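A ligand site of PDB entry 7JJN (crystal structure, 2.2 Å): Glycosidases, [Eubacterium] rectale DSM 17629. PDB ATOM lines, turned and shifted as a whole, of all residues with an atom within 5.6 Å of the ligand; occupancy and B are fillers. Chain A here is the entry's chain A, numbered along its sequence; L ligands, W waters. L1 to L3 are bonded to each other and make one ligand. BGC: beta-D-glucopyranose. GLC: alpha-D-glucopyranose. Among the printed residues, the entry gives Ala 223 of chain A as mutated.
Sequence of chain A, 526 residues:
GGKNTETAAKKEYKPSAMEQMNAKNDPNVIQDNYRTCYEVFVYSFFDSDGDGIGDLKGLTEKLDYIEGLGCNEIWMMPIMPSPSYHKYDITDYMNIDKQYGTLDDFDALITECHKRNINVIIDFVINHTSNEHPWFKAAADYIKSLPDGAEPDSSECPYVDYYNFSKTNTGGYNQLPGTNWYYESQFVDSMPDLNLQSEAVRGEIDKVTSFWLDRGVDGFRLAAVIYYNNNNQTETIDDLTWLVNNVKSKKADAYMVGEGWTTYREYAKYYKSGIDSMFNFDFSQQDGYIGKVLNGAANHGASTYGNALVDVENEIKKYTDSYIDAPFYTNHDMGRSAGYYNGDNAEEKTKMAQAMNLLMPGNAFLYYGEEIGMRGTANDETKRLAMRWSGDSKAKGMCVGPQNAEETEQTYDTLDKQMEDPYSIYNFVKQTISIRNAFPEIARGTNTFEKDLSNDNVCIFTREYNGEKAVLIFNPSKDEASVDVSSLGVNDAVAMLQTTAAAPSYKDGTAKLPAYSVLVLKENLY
The guanidinium group (NH2) of Arg 221 lies within hydrogen-bond range of an oxygen (O2) of BGC L1 (3.0 Å). A ring nitrogen (NE2) of His 332 lies within hydrogen-bond range of an oxygen (O2) of BGC L1, 2.9 Å away. OD2 of Asp 333 sits at hydrogen-bond distance from O2 of BGC L1, at 2.5 Å. OE1 of Glu 259 sits at hydrogen-bond distance from O1 of BGC L1, at 2.5 Å. NH2 of Arg 384 is in hydrogen-bond range of O2 of GLC L2 (2.9 Å). NE2 of His 128 is in hydrogen-bond range of O6 of BGC L1, 3.0 Å away. O2 of GLC L3 lies within hydrogen-bond range of OD2 of Asp 380, 2.6 Å away.
CE1 of His 86 touches C2 of GLC L2 (3.8 Å). CB of Tyr 88 touches O6 of BGC L1, 3.4 Å away. CD1 of Phe 187 touches C6 of BGC L1, 3.8 Å away. CG1 of Val 188 touches O6 of GLC L2, at 3.7 Å. CE of Met 191 touches O5 of GLC L2, 3.6 Å away. CB of Ala 223 touches O1 of BGC L1 (3.2 Å). N of Ala 224 touches O1 of BGC L1, 3.7 Å away. Hydrophobic or aromatic side chains that line the ligand: His 86, Tyr 88, His 128, Phe 187, Val 188, Met 191, Ala 223 and His 332. The nearest printed residue that does not touch the ligand is Tyr 85 (4.5 Å).
The backbone NH (N) of Tyr 88 is in hydrogen-bond range of a ring nitrogen (ND1) of His 86, 3.2 Å away. OE1 of Glu 259 sits at hydrogen-bond distance from N of Ala 224. OH of Tyr 88 lies within hydrogen-bond range of NE2 of His 332 (3.0 Å). OD2 of Asp 380 lies within salt-bridge range of NH2 of Arg 384 (3.9 Å). The guanidinium group (NH2) of Arg 221 lies within salt-bridge range of the side-chain carboxylate (OE1) of Glu 259, at 3.4 Å. The guanidinium group (NH1) of Arg 221 is in hydrogen-bond range of the side-chain hydroxyl (OH) of Tyr 88 (3.3 Å). O of His 332 lies within hydrogen-bond range of NE of Arg 384, at 2.8 Å. OH of Tyr 88 is in hydrogen-bond range of OD2 of Asp 123.
Water W4 lies within hydrogen-bond range of OH of Tyr 85 (2.7 Å) and O3 of GLC L2 (2.7 Å). Water W3 lies within hydrogen-bond range of an oxygen (O6) of GLC L2 and a ring nitrogen (NE2) of His 86. Water W5 lies within hydrogen-bond range of OD1 of Asp 380 and O3 of GLC L3. Water W7 lies within hydrogen-bond range of OD1 of Asn 127 (2.8 Å), O6 of BGC L1 (2.8 Å) and NE2 of His 128 (3.3 Å). Water W2 lies within hydrogen-bond range of an oxygen (O2) of GLC L3 and the backbone NH (N) of Asp 380. Water W6 bridges OE2 of Glu 259 (2.9 Å) and OD2 of Asp 333 (3.0 Å).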
ATOM      1  N   TYR A  85      -3.567  13.034  -0.340  1.00  0.00           N
ATOM      2  CA  TYR A  85      -2.189  13.332  -0.744  1.00  0.00           C
ATOM      3  C   TYR A  85      -2.164  13.973  -2.136  1.00  0.00           C
ATOM      4  O   TYR A  85      -1.262  14.757  -2.442  1.00  0.00           O
ATOM      5  CB  TYR A  85      -1.318  12.055  -0.718  1.00  0.00           C
ATOM      6  CG  TYR A  85      -1.473  11.178  -1.934  1.00  0.00           C
ATOM      7  CD1 TYR A  85      -2.540  10.309  -2.058  1.00  0.00           C
ATOM      8  CD2 TYR A  85      -0.587  11.271  -2.995  1.00  0.00           C
ATOM      9  CE1 TYR A  85      -2.712   9.541  -3.202  1.00  0.00           C
ATOM     10  CE2 TYR A  85      -0.734  10.504  -4.139  1.00  0.00           C
ATOM     11  CZ  TYR A  85      -1.813   9.639  -4.245  1.00  0.00           C
ATOM     12  OH  TYR A  85      -1.965   8.891  -5.380  1.00  0.00           O
ATOM     13  N   HIS A  86      -3.135  13.635  -2.988  1.00  0.00           N
ATOM     14  CA  HIS A  86      -3.093  14.013  -4.396  1.00  0.00           C
ATOM     15  C   HIS A  86      -3.772  15.380  -4.595  1.00  0.00           C
ATOM     16  O   HIS A  86      -3.357  16.138  -5.476  1.00  0.00           O
ATOM     17  CB  HIS A  86      -3.688  12.915  -5.278  1.00  0.00           C
ATOM     18  CG  HIS A  86      -5.084  12.535  -4.946  1.00  0.00           C
ATOM     19  ND1 HIS A  86      -6.149  13.312  -5.290  1.00  0.00           N
ATOM     20  CD2 HIS A  86      -5.579  11.457  -4.321  1.00  0.00           C
ATOM     21  CE1 HIS A  86      -7.256  12.744  -4.871  1.00  0.00           C
ATOM     22  NE2 HIS A  86      -6.930  11.606  -4.259  1.00  0.00           N
ATOM     23  N   TYR A  88      -6.942  16.403  -5.399  1.00  0.00           N
ATOM     24  CA  TYR A  88      -8.003  16.630  -6.387  1.00  0.00           C
ATOM     25  C   TYR A  88      -9.386  16.797  -5.729  1.00  0.00           C
ATOM     26  O   TYR A  88     -10.304  17.250  -6.402  1.00  0.00           O
ATOM     27  CB  TYR A  88      -7.987  15.502  -7.434  1.00  0.00           C
ATOM     28  CG  TYR A  88      -6.970  15.762  -8.512  1.00  0.00           C
ATOM     29  CD1 TYR A  88      -7.251  16.629  -9.545  1.00  0.00           C
ATOM     30  CD2 TYR A  88      -5.714  15.196  -8.471  1.00  0.00           C
ATOM     31  CE1 TYR A  88      -6.327  16.919 -10.533  1.00  0.00           C
ATOM     32  CE2 TYR A  88      -4.761  15.465  -9.452  1.00  0.00           C
ATOM     33  CZ  TYR A  88      -5.078  16.324 -10.486  1.00  0.00           C
ATOM     34  OH  TYR A  88      -4.166  16.618 -11.456  1.00  0.00           O
ATOM     35  N   ASP A  89      -9.524  16.478  -4.443  1.00  0.00           N
ATOM     36  CA  ASP A  89     -10.769  16.692  -3.682  1.00  0.00           C
ATOM     37  C   ASP A  89     -10.575  17.899  -2.746  1.00  0.00           C
ATOM     38  O   ASP A  89      -9.923  17.767  -1.711  1.00  0.00           O
ATOM     39  CB  ASP A  89     -11.165  15.438  -2.879  1.00  0.00           C
ATOM     40  CG  ASP A  89     -10.054  14.784  -2.064  1.00  0.00           C
ATOM     41  OD1 ASP A  89      -8.858  14.880  -2.467  1.00  0.00           O
ATOM     42  OD2 ASP A  89     -10.371  14.183  -1.025  1.00  0.00           O
ATOM     43  N   ASP A 123      -3.897  23.582 -11.588  1.00  0.00           N
ATOM     44  CA  ASP A 123      -4.934  22.581 -11.771  1.00  0.00           C
ATOM     45  C   ASP A 123      -6.237  23.147 -11.194  1.00  0.00           C
ATOM     46  O   ASP A 123      -6.287  23.523 -10.045  1.00  0.00           O
ATOM     47  CB  ASP A 123      -4.529  21.249 -11.136  1.00  0.00           C
ATOM     48  CG  ASP A 123      -5.032  20.031 -11.876  1.00  0.00           C
ATOM     49  OD1 ASP A 123      -6.256  19.998 -12.189  1.00  0.00           O
ATOM     50  OD2 ASP A 123      -4.200  19.127 -12.155  1.00  0.00           O
ATOM     51  N   VAL A 125     -10.064  22.380 -10.563  1.00  0.00           N
ATOM     52  CA  VAL A 125     -10.896  21.222 -10.363  1.00  0.00           C
ATOM     53  C   VAL A 125     -12.271  21.691  -9.907  1.00  0.00           C
ATOM     54  O   VAL A 125     -12.466  21.906  -8.698  1.00  0.00           O
ATOM     55  CB  VAL A 125     -10.251  20.260  -9.346  1.00  0.00           C
ATOM     56  CG1 VAL A 125     -11.013  18.952  -9.250  1.00  0.00           C
ATOM     57  CG2 VAL A 125      -8.791  20.022  -9.655  1.00  0.00           C
ATOM     58  N   ASN A 127     -15.295  20.226 -11.452  1.00  0.00           N
ATOM     59  CA  ASN A 127     -16.334  19.225 -11.723  1.00  0.00           C
ATOM     60  C   ASN A 127     -16.888  18.657 -10.395  1.00  0.00           C
ATOM     61  O   ASN A 127     -18.045  18.188 -10.362  1.00  0.00           O
ATOM     62  CB  ASN A 127     -15.860  18.088 -12.628  1.00  0.00           C
ATOM     63  CG  ASN A 127     -14.784  17.233 -11.998  1.00  0.00           C
ATOM     64  OD1 ASN A 127     -13.670  17.699 -11.767  1.00  0.00           O
ATOM     65  ND2 ASN A 127     -15.103  15.969 -11.785  1.00  0.00           N
ATOM     66  N   HIS A 128     -16.058  18.667  -9.342  1.00  0.00           N
ATOM     67  CA  HIS A 128     -16.450  18.214  -8.012  1.00  0.00           C
ATOM     68  C   HIS A 128     -15.666  18.966  -6.943  1.00  0.00           C
ATOM     69  O   HIS A 128     -14.689  19.642  -7.229  1.00  0.00           O
ATOM     70  CB  HIS A 128     -16.320  16.688  -7.870  1.00  0.00           C
ATOM     71  CG  HIS A 128     -14.986  16.110  -8.203  1.00  0.00           C
ATOM     72  ND1 HIS A 128     -13.801  16.648  -7.746  1.00  0.00           N
ATOM     73  CD2 HIS A 128     -14.656  15.003  -8.905  1.00  0.00           C
ATOM     74  CE1 HIS A 128     -12.788  15.913  -8.172  1.00  0.00           C
ATOM     75  NE2 HIS A 128     -13.285  14.905  -8.883  1.00  0.00           N
ATOM     76  N   PHE A 187     -16.964  10.029  -9.467  1.00  0.00           N
ATOM     77  CA  PHE A 187     -15.626   9.469  -9.224  1.00  0.00           C
ATOM     78  C   PHE A 187     -15.621   8.574  -7.975  1.00  0.00           C
ATOM     79  O   PHE A 187     -15.051   7.485  -8.001  1.00  0.00           O
ATOM     80  CB  PHE A 187     -14.568  10.569  -9.153  1.00  0.00           C
ATOM     81  CG  PHE A 187     -14.091  11.022 -10.504  1.00  0.00           C
ATOM     82  CD1 PHE A 187     -13.070  10.341 -11.155  1.00  0.00           C
ATOM     83  CD2 PHE A 187     -14.684  12.096 -11.153  1.00  0.00           C
ATOM     84  CE1 PHE A 187     -12.645  10.734 -12.415  1.00  0.00           C
ATOM     85  CE2 PHE A 187     -14.247  12.496 -12.411  1.00  0.00           C
ATOM     86  CZ  PHE A 187     -13.233  11.813 -13.051  1.00  0.00           C
ATOM     87  N   VAL A 188     -16.254   9.042  -6.897  1.00  0.00           N
ATOM     88  CA  VAL A 188     -16.289   8.325  -5.606  1.00  0.00           C
ATOM     89  C   VAL A 188     -17.147   9.162  -4.640  1.00  0.00           C
ATOM     90  O   VAL A 188     -17.357  10.351  -4.895  1.00  0.00           O
ATOM     91  CB  VAL A 188     -14.858   8.085  -5.071  1.00  0.00           C
ATOM     92  CG1 VAL A 188     -14.075   9.375  -4.965  1.00  0.00           C
ATOM     93  CG2 VAL A 188     -14.838   7.317  -3.760  1.00  0.00           C
ATOM     94  N   MET A 191     -16.286  12.667  -3.360  1.00  0.00           N
ATOM     95  CA  MET A 191     -16.125  13.709  -4.373  1.00  0.00           C
ATOM     96  C   MET A 191     -17.498  14.065  -4.983  1.00  0.00           C
ATOM     97  O   MET A 191     -17.808  13.684  -6.116  1.00  0.00           O
ATOM     98  CB  MET A 191     -15.141  13.243  -5.455  1.00  0.00           C
ATOM     99  CG  MET A 191     -13.676  13.196  -4.988  1.00  0.00           C
ATOM    100  SD  MET A 191     -12.527  12.726  -6.340  1.00  0.00           S
ATOM    101  CE  MET A 191     -10.973  13.457  -5.821  1.00  0.00           C
ATOM    102  N   ARG A 221      -5.200  24.336 -16.029  1.00  0.00           N
ATOM    103  CA  ARG A 221      -5.510  22.990 -16.475  1.00  0.00           C
ATOM    104  C   ARG A 221      -6.884  22.613 -15.904  1.00  0.00           C
ATOM    105  O   ARG A 221      -7.076  22.609 -14.668  1.00  0.00           O
ATOM    106  CB  ARG A 221      -4.392  22.029 -16.046  1.00  0.00           C
ATOM    107  CG  ARG A 221      -4.564  20.602 -16.528  1.00  0.00           C
ATOM    108  CD  ARG A 221      -5.218  19.700 -15.500  1.00  0.00           C
ATOM    109  NE  ARG A 221      -5.244  18.280 -15.856  1.00  0.00           N
ATOM    110  CZ  ARG A 221      -5.750  17.319 -15.077  1.00  0.00           C
ATOM    111  NH1 ARG A 221      -6.178  17.608 -13.855  1.00  0.00           N
ATOM    112  NH2 ARG A 221      -5.844  16.071 -15.531  1.00  0.00           N
ATOM    113  N   ALA A 223      -9.569  20.077 -15.034  1.00  0.00           N
ATOM    114  CA  ALA A 223      -9.744  18.670 -14.745  1.00  0.00           C
ATOM    115  C   ALA A 223     -11.147  18.246 -15.170  1.00  0.00           C
ATOM    116  O   ALA A 223     -12.115  18.959 -14.943  1.00  0.00           O
ATOM    117  CB  ALA A 223      -9.533  18.400 -13.274  1.00  0.00           C
ATOM    118  N   ALA A 224     -11.213  17.069 -15.824  1.00  0.00           N
ATOM    119  CA  ALA A 224     -12.413  16.287 -16.029  1.00  0.00           C
ATOM    120  C   ALA A 224     -13.465  17.082 -16.811  1.00  0.00           C
ATOM    121  O   ALA A 224     -14.654  17.047 -16.468  1.00  0.00           O
ATOM    122  CB  ALA A 224     -12.940  15.845 -14.676  1.00  0.00           C
ATOM    123  N   GLU A 259      -8.684  18.475 -19.879  1.00  0.00           N
ATOM    124  CA  GLU A 259      -8.516  17.044 -19.822  1.00  0.00           C
ATOM    125  C   GLU A 259      -9.820  16.344 -20.244  1.00  0.00           C
ATOM    126  O   GLU A 259     -10.792  16.274 -19.469  1.00  0.00           O
ATOM    127  CB  GLU A 259      -8.115  16.629 -18.417  1.00  0.00           C
ATOM    128  CG  GLU A 259      -7.796  15.152 -18.301  1.00  0.00           C
ATOM    129  CD  GLU A 259      -8.265  14.496 -17.021  1.00  0.00           C
ATOM    130  OE1 GLU A 259      -9.055  15.117 -16.252  1.00  0.00           O
ATOM    131  OE2 GLU A 259      -7.830  13.364 -16.792  1.00  0.00           O
ATOM    132  N   HIS A 332       0.326  11.993 -14.560  1.00  0.00           N
ATOM    133  CA  HIS A 332       0.201  11.459 -13.187  1.00  0.00           C
ATOM    134  C   HIS A 332      -0.882  10.373 -13.055  1.00  0.00           C
ATOM    135  O   HIS A 332      -0.978   9.777 -11.987  1.00  0.00           O
ATOM    136  CB  HIS A 332      -0.105  12.602 -12.229  1.00  0.00           C
ATOM    137  CG  HIS A 332      -1.386  13.293 -12.546  1.00  0.00           C
ATOM    138  ND1 HIS A 332      -1.470  14.278 -13.501  1.00  0.00           N
ATOM    139  CD2 HIS A 332      -2.640  13.084 -12.084  1.00  0.00           C
ATOM    140  CE1 HIS A 332      -2.720  14.682 -13.604  1.00  0.00           C
ATOM    141  NE2 HIS A 332      -3.452  13.960 -12.730  1.00  0.00           N
ATOM    142  N   ASP A 333      -1.697  10.167 -14.095  1.00  0.00           N
ATOM    143  CA  ASP A 333      -2.758   9.170 -14.095  1.00  0.00           C
ATOM    144  C   ASP A 333      -2.352   7.897 -14.856  1.00  0.00           C
ATOM    145  O   ASP A 333      -3.113   6.931 -14.872  1.00  0.00           O
ATOM    146  CB  ASP A 333      -4.041   9.729 -14.733  1.00  0.00           C
ATOM    147  CG  ASP A 333      -4.751  10.754 -13.863  1.00  0.00           C
ATOM    148  OD1 ASP A 333      -4.623  10.643 -12.633  1.00  0.00           O
ATOM    149  OD2 ASP A 333      -5.378  11.660 -14.423  1.00  0.00           O
ATOM    150  N   ASP A 380      -2.004   4.336  -8.703  1.00  0.00           N
ATOM    151  CA  ASP A 380      -1.874   5.772  -8.956  1.00  0.00           C
ATOM    152  C   ASP A 380      -0.726   6.335  -8.113  1.00  0.00           C
ATOM    153  O   ASP A 380       0.118   7.051  -8.628  1.00  0.00           O
ATOM    154  CB  ASP A 380      -3.198   6.507  -8.749  1.00  0.00           C
ATOM    155  CG  ASP A 380      -4.213   6.334  -9.865  1.00  0.00           C
ATOM    156  OD1 ASP A 380      -3.885   5.679 -10.900  1.00  0.00           O
ATOM    157  OD2 ASP A 380      -5.348   6.844  -9.713  1.00  0.00           O
ATOM    158  N   GLU A 381      -0.674   5.982  -6.827  1.00  0.00           N
ATOM    159  CA  GLU A 381       0.393   6.414  -5.909  1.00  0.00           C
ATOM    160  C   GLU A 381       1.771   6.143  -6.514  1.00  0.00           C
ATOM    161  O   GLU A 381       2.693   6.952  -6.413  1.00  0.00           O
ATOM    162  CB  GLU A 381       0.274   5.676  -4.565  1.00  0.00           C
ATOM    163  CG  GLU A 381      -0.922   6.092  -3.713  1.00  0.00           C
ATOM    164  CD  GLU A 381      -2.228   5.331  -3.900  1.00  0.00           C
ATOM    165  OE1 GLU A 381      -2.345   4.522  -4.876  1.00  0.00           O
ATOM    166  OE2 GLU A 381      -3.140   5.540  -3.062  1.00  0.00           O
ATOM    167  N   ARG A 384       3.466   8.417  -8.984  1.00  0.00           N
ATOM    168  CA  ARG A 384       3.740   9.740  -8.412  1.00  0.00           C
ATOM    169  C   ARG A 384       4.840   9.652  -7.343  1.00  0.00           C
ATOM    170  O   ARG A 384       4.784  10.343  -6.316  1.00  0.00           O
ATOM    171  CB  ARG A 384       2.433  10.287  -7.850  1.00  0.00           C
ATOM    172  CG  ARG A 384       1.292  10.313  -8.864  1.00  0.00           C
ATOM    173  CD  ARG A 384      -0.078  10.380  -8.200  1.00  0.00           C
ATOM    174  NE  ARG A 384      -1.098  10.270  -9.228  1.00  0.00           N
ATOM    175  CZ  ARG A 384      -2.395  10.234  -8.994  1.00  0.00           C
ATOM    176  NH1 ARG A 384      -2.856  10.375  -7.755  1.00  0.00           N
ATOM    177  NH2 ARG A 384      -3.228  10.066 -10.004  1.00  0.00           N
HETATM  178  C2  BGC L   1      -7.171  13.930 -12.517  1.00  0.00           C
HETATM  179  C3  BGC L   1      -7.111  12.633 -11.719  1.00  0.00           C
HETATM  180  C4  BGC L   1      -8.152  12.711 -10.607  1.00  0.00           C
HETATM  181  C5  BGC L   1      -9.531  12.931 -11.223  1.00  0.00           C
HETATM  182  C6  BGC L   1     -10.626  13.087 -10.165  1.00  0.00           C
HETATM  183  C1  BGC L   1      -8.575  14.118 -13.079  1.00  0.00           C
HETATM  184  O1  BGC L   1      -8.666  15.357 -13.763  1.00  0.00           O
HETATM  185  O2  BGC L   1      -6.199  13.889 -13.574  1.00  0.00           O
HETATM  186  O3  BGC L   1      -5.820  12.427 -11.168  1.00  0.00           O
HETATM  187  O4  BGC L   1      -8.117  11.463  -9.893  1.00  0.00           O
HETATM  188  O5  BGC L   1      -9.528  14.115 -12.019  1.00  0.00           O
HETATM  189  O6  BGC L   1     -10.439  14.317  -9.454  1.00  0.00           O
HETATM  190  C1  GLC L   2      -7.970  11.551  -8.471  1.00  0.00           C
HETATM  191  C2  GLC L   2      -6.754  10.764  -8.028  1.00  0.00           C
HETATM  192  C3  GLC L   2      -6.934   9.270  -8.286  1.00  0.00           C
HETATM  193  C4  GLC L   2      -8.227   8.770  -7.650  1.00  0.00           C
HETATM  194  C5  GLC L   2      -9.410   9.672  -8.040  1.00  0.00           C
HETATM  195  C6  GLC L   2     -10.703   9.295  -7.318  1.00  0.00           C
HETATM  196  O2  GLC L   2      -5.585  11.251  -8.715  1.00  0.00           O
HETATM  197  O3  GLC L   2      -5.798   8.560  -7.769  1.00  0.00           O
HETATM  198  O4  GLC L   2      -8.498   7.444  -8.117  1.00  0.00           O
HETATM  199  O5  GLC L   2      -9.118  11.056  -7.780  1.00  0.00           O
HETATM  200  O6  GLC L   2     -10.538   9.276  -5.897  1.00  0.00           O
HETATM  201  C1  GLC L   3      -8.566   6.452  -7.076  1.00  0.00           C
HETATM  202  C2  GLC L   3      -7.847   5.194  -7.546  1.00  0.00           C
HETATM  203  C3  GLC L   3      -8.530   4.634  -8.785  1.00  0.00           C
HETATM  204  C4  GLC L   3      -9.949   4.258  -8.399  1.00  0.00           C
HETATM  205  C5  GLC L   3     -10.675   5.457  -7.798  1.00  0.00           C
HETATM  206  C6  GLC L   3     -12.048   5.030  -7.270  1.00  0.00           C
HETATM  207  O2  GLC L   3      -6.461   5.489  -7.798  1.00  0.00           O
HETATM  208  O3  GLC L   3      -7.838   3.489  -9.293  1.00  0.00           O
HETATM  209  O4  GLC L   3     -10.631   3.778  -9.560  1.00  0.00           O
HETATM  210  O5  GLC L   3      -9.909   6.080  -6.733  1.00  0.00           O
HETATM  211  O6  GLC L   3     -12.265   5.502  -5.930  1.00  0.00           O
HETATM  212  O   HOH W   1     -11.330   2.920 -11.967  1.00  0.00           O
HETATM  213  O   HOH W   2      -4.784   3.178  -8.060  1.00  0.00           O
HETATM  214  O   HOH W   3      -9.441   9.958  -3.491  1.00  0.00           O
HETATM  215  O   HOH W   4      -4.457   7.912  -5.501  1.00  0.00           O
HETATM  216  O   HOH W   5      -5.909   3.910 -11.228  1.00  0.00           O
HETATM  217  O   HOH W   6      -8.273  11.197 -14.901  1.00  0.00           O
HETATM  218  O   HOH W   7     -11.413  16.101 -11.383  1.00  0.00           O
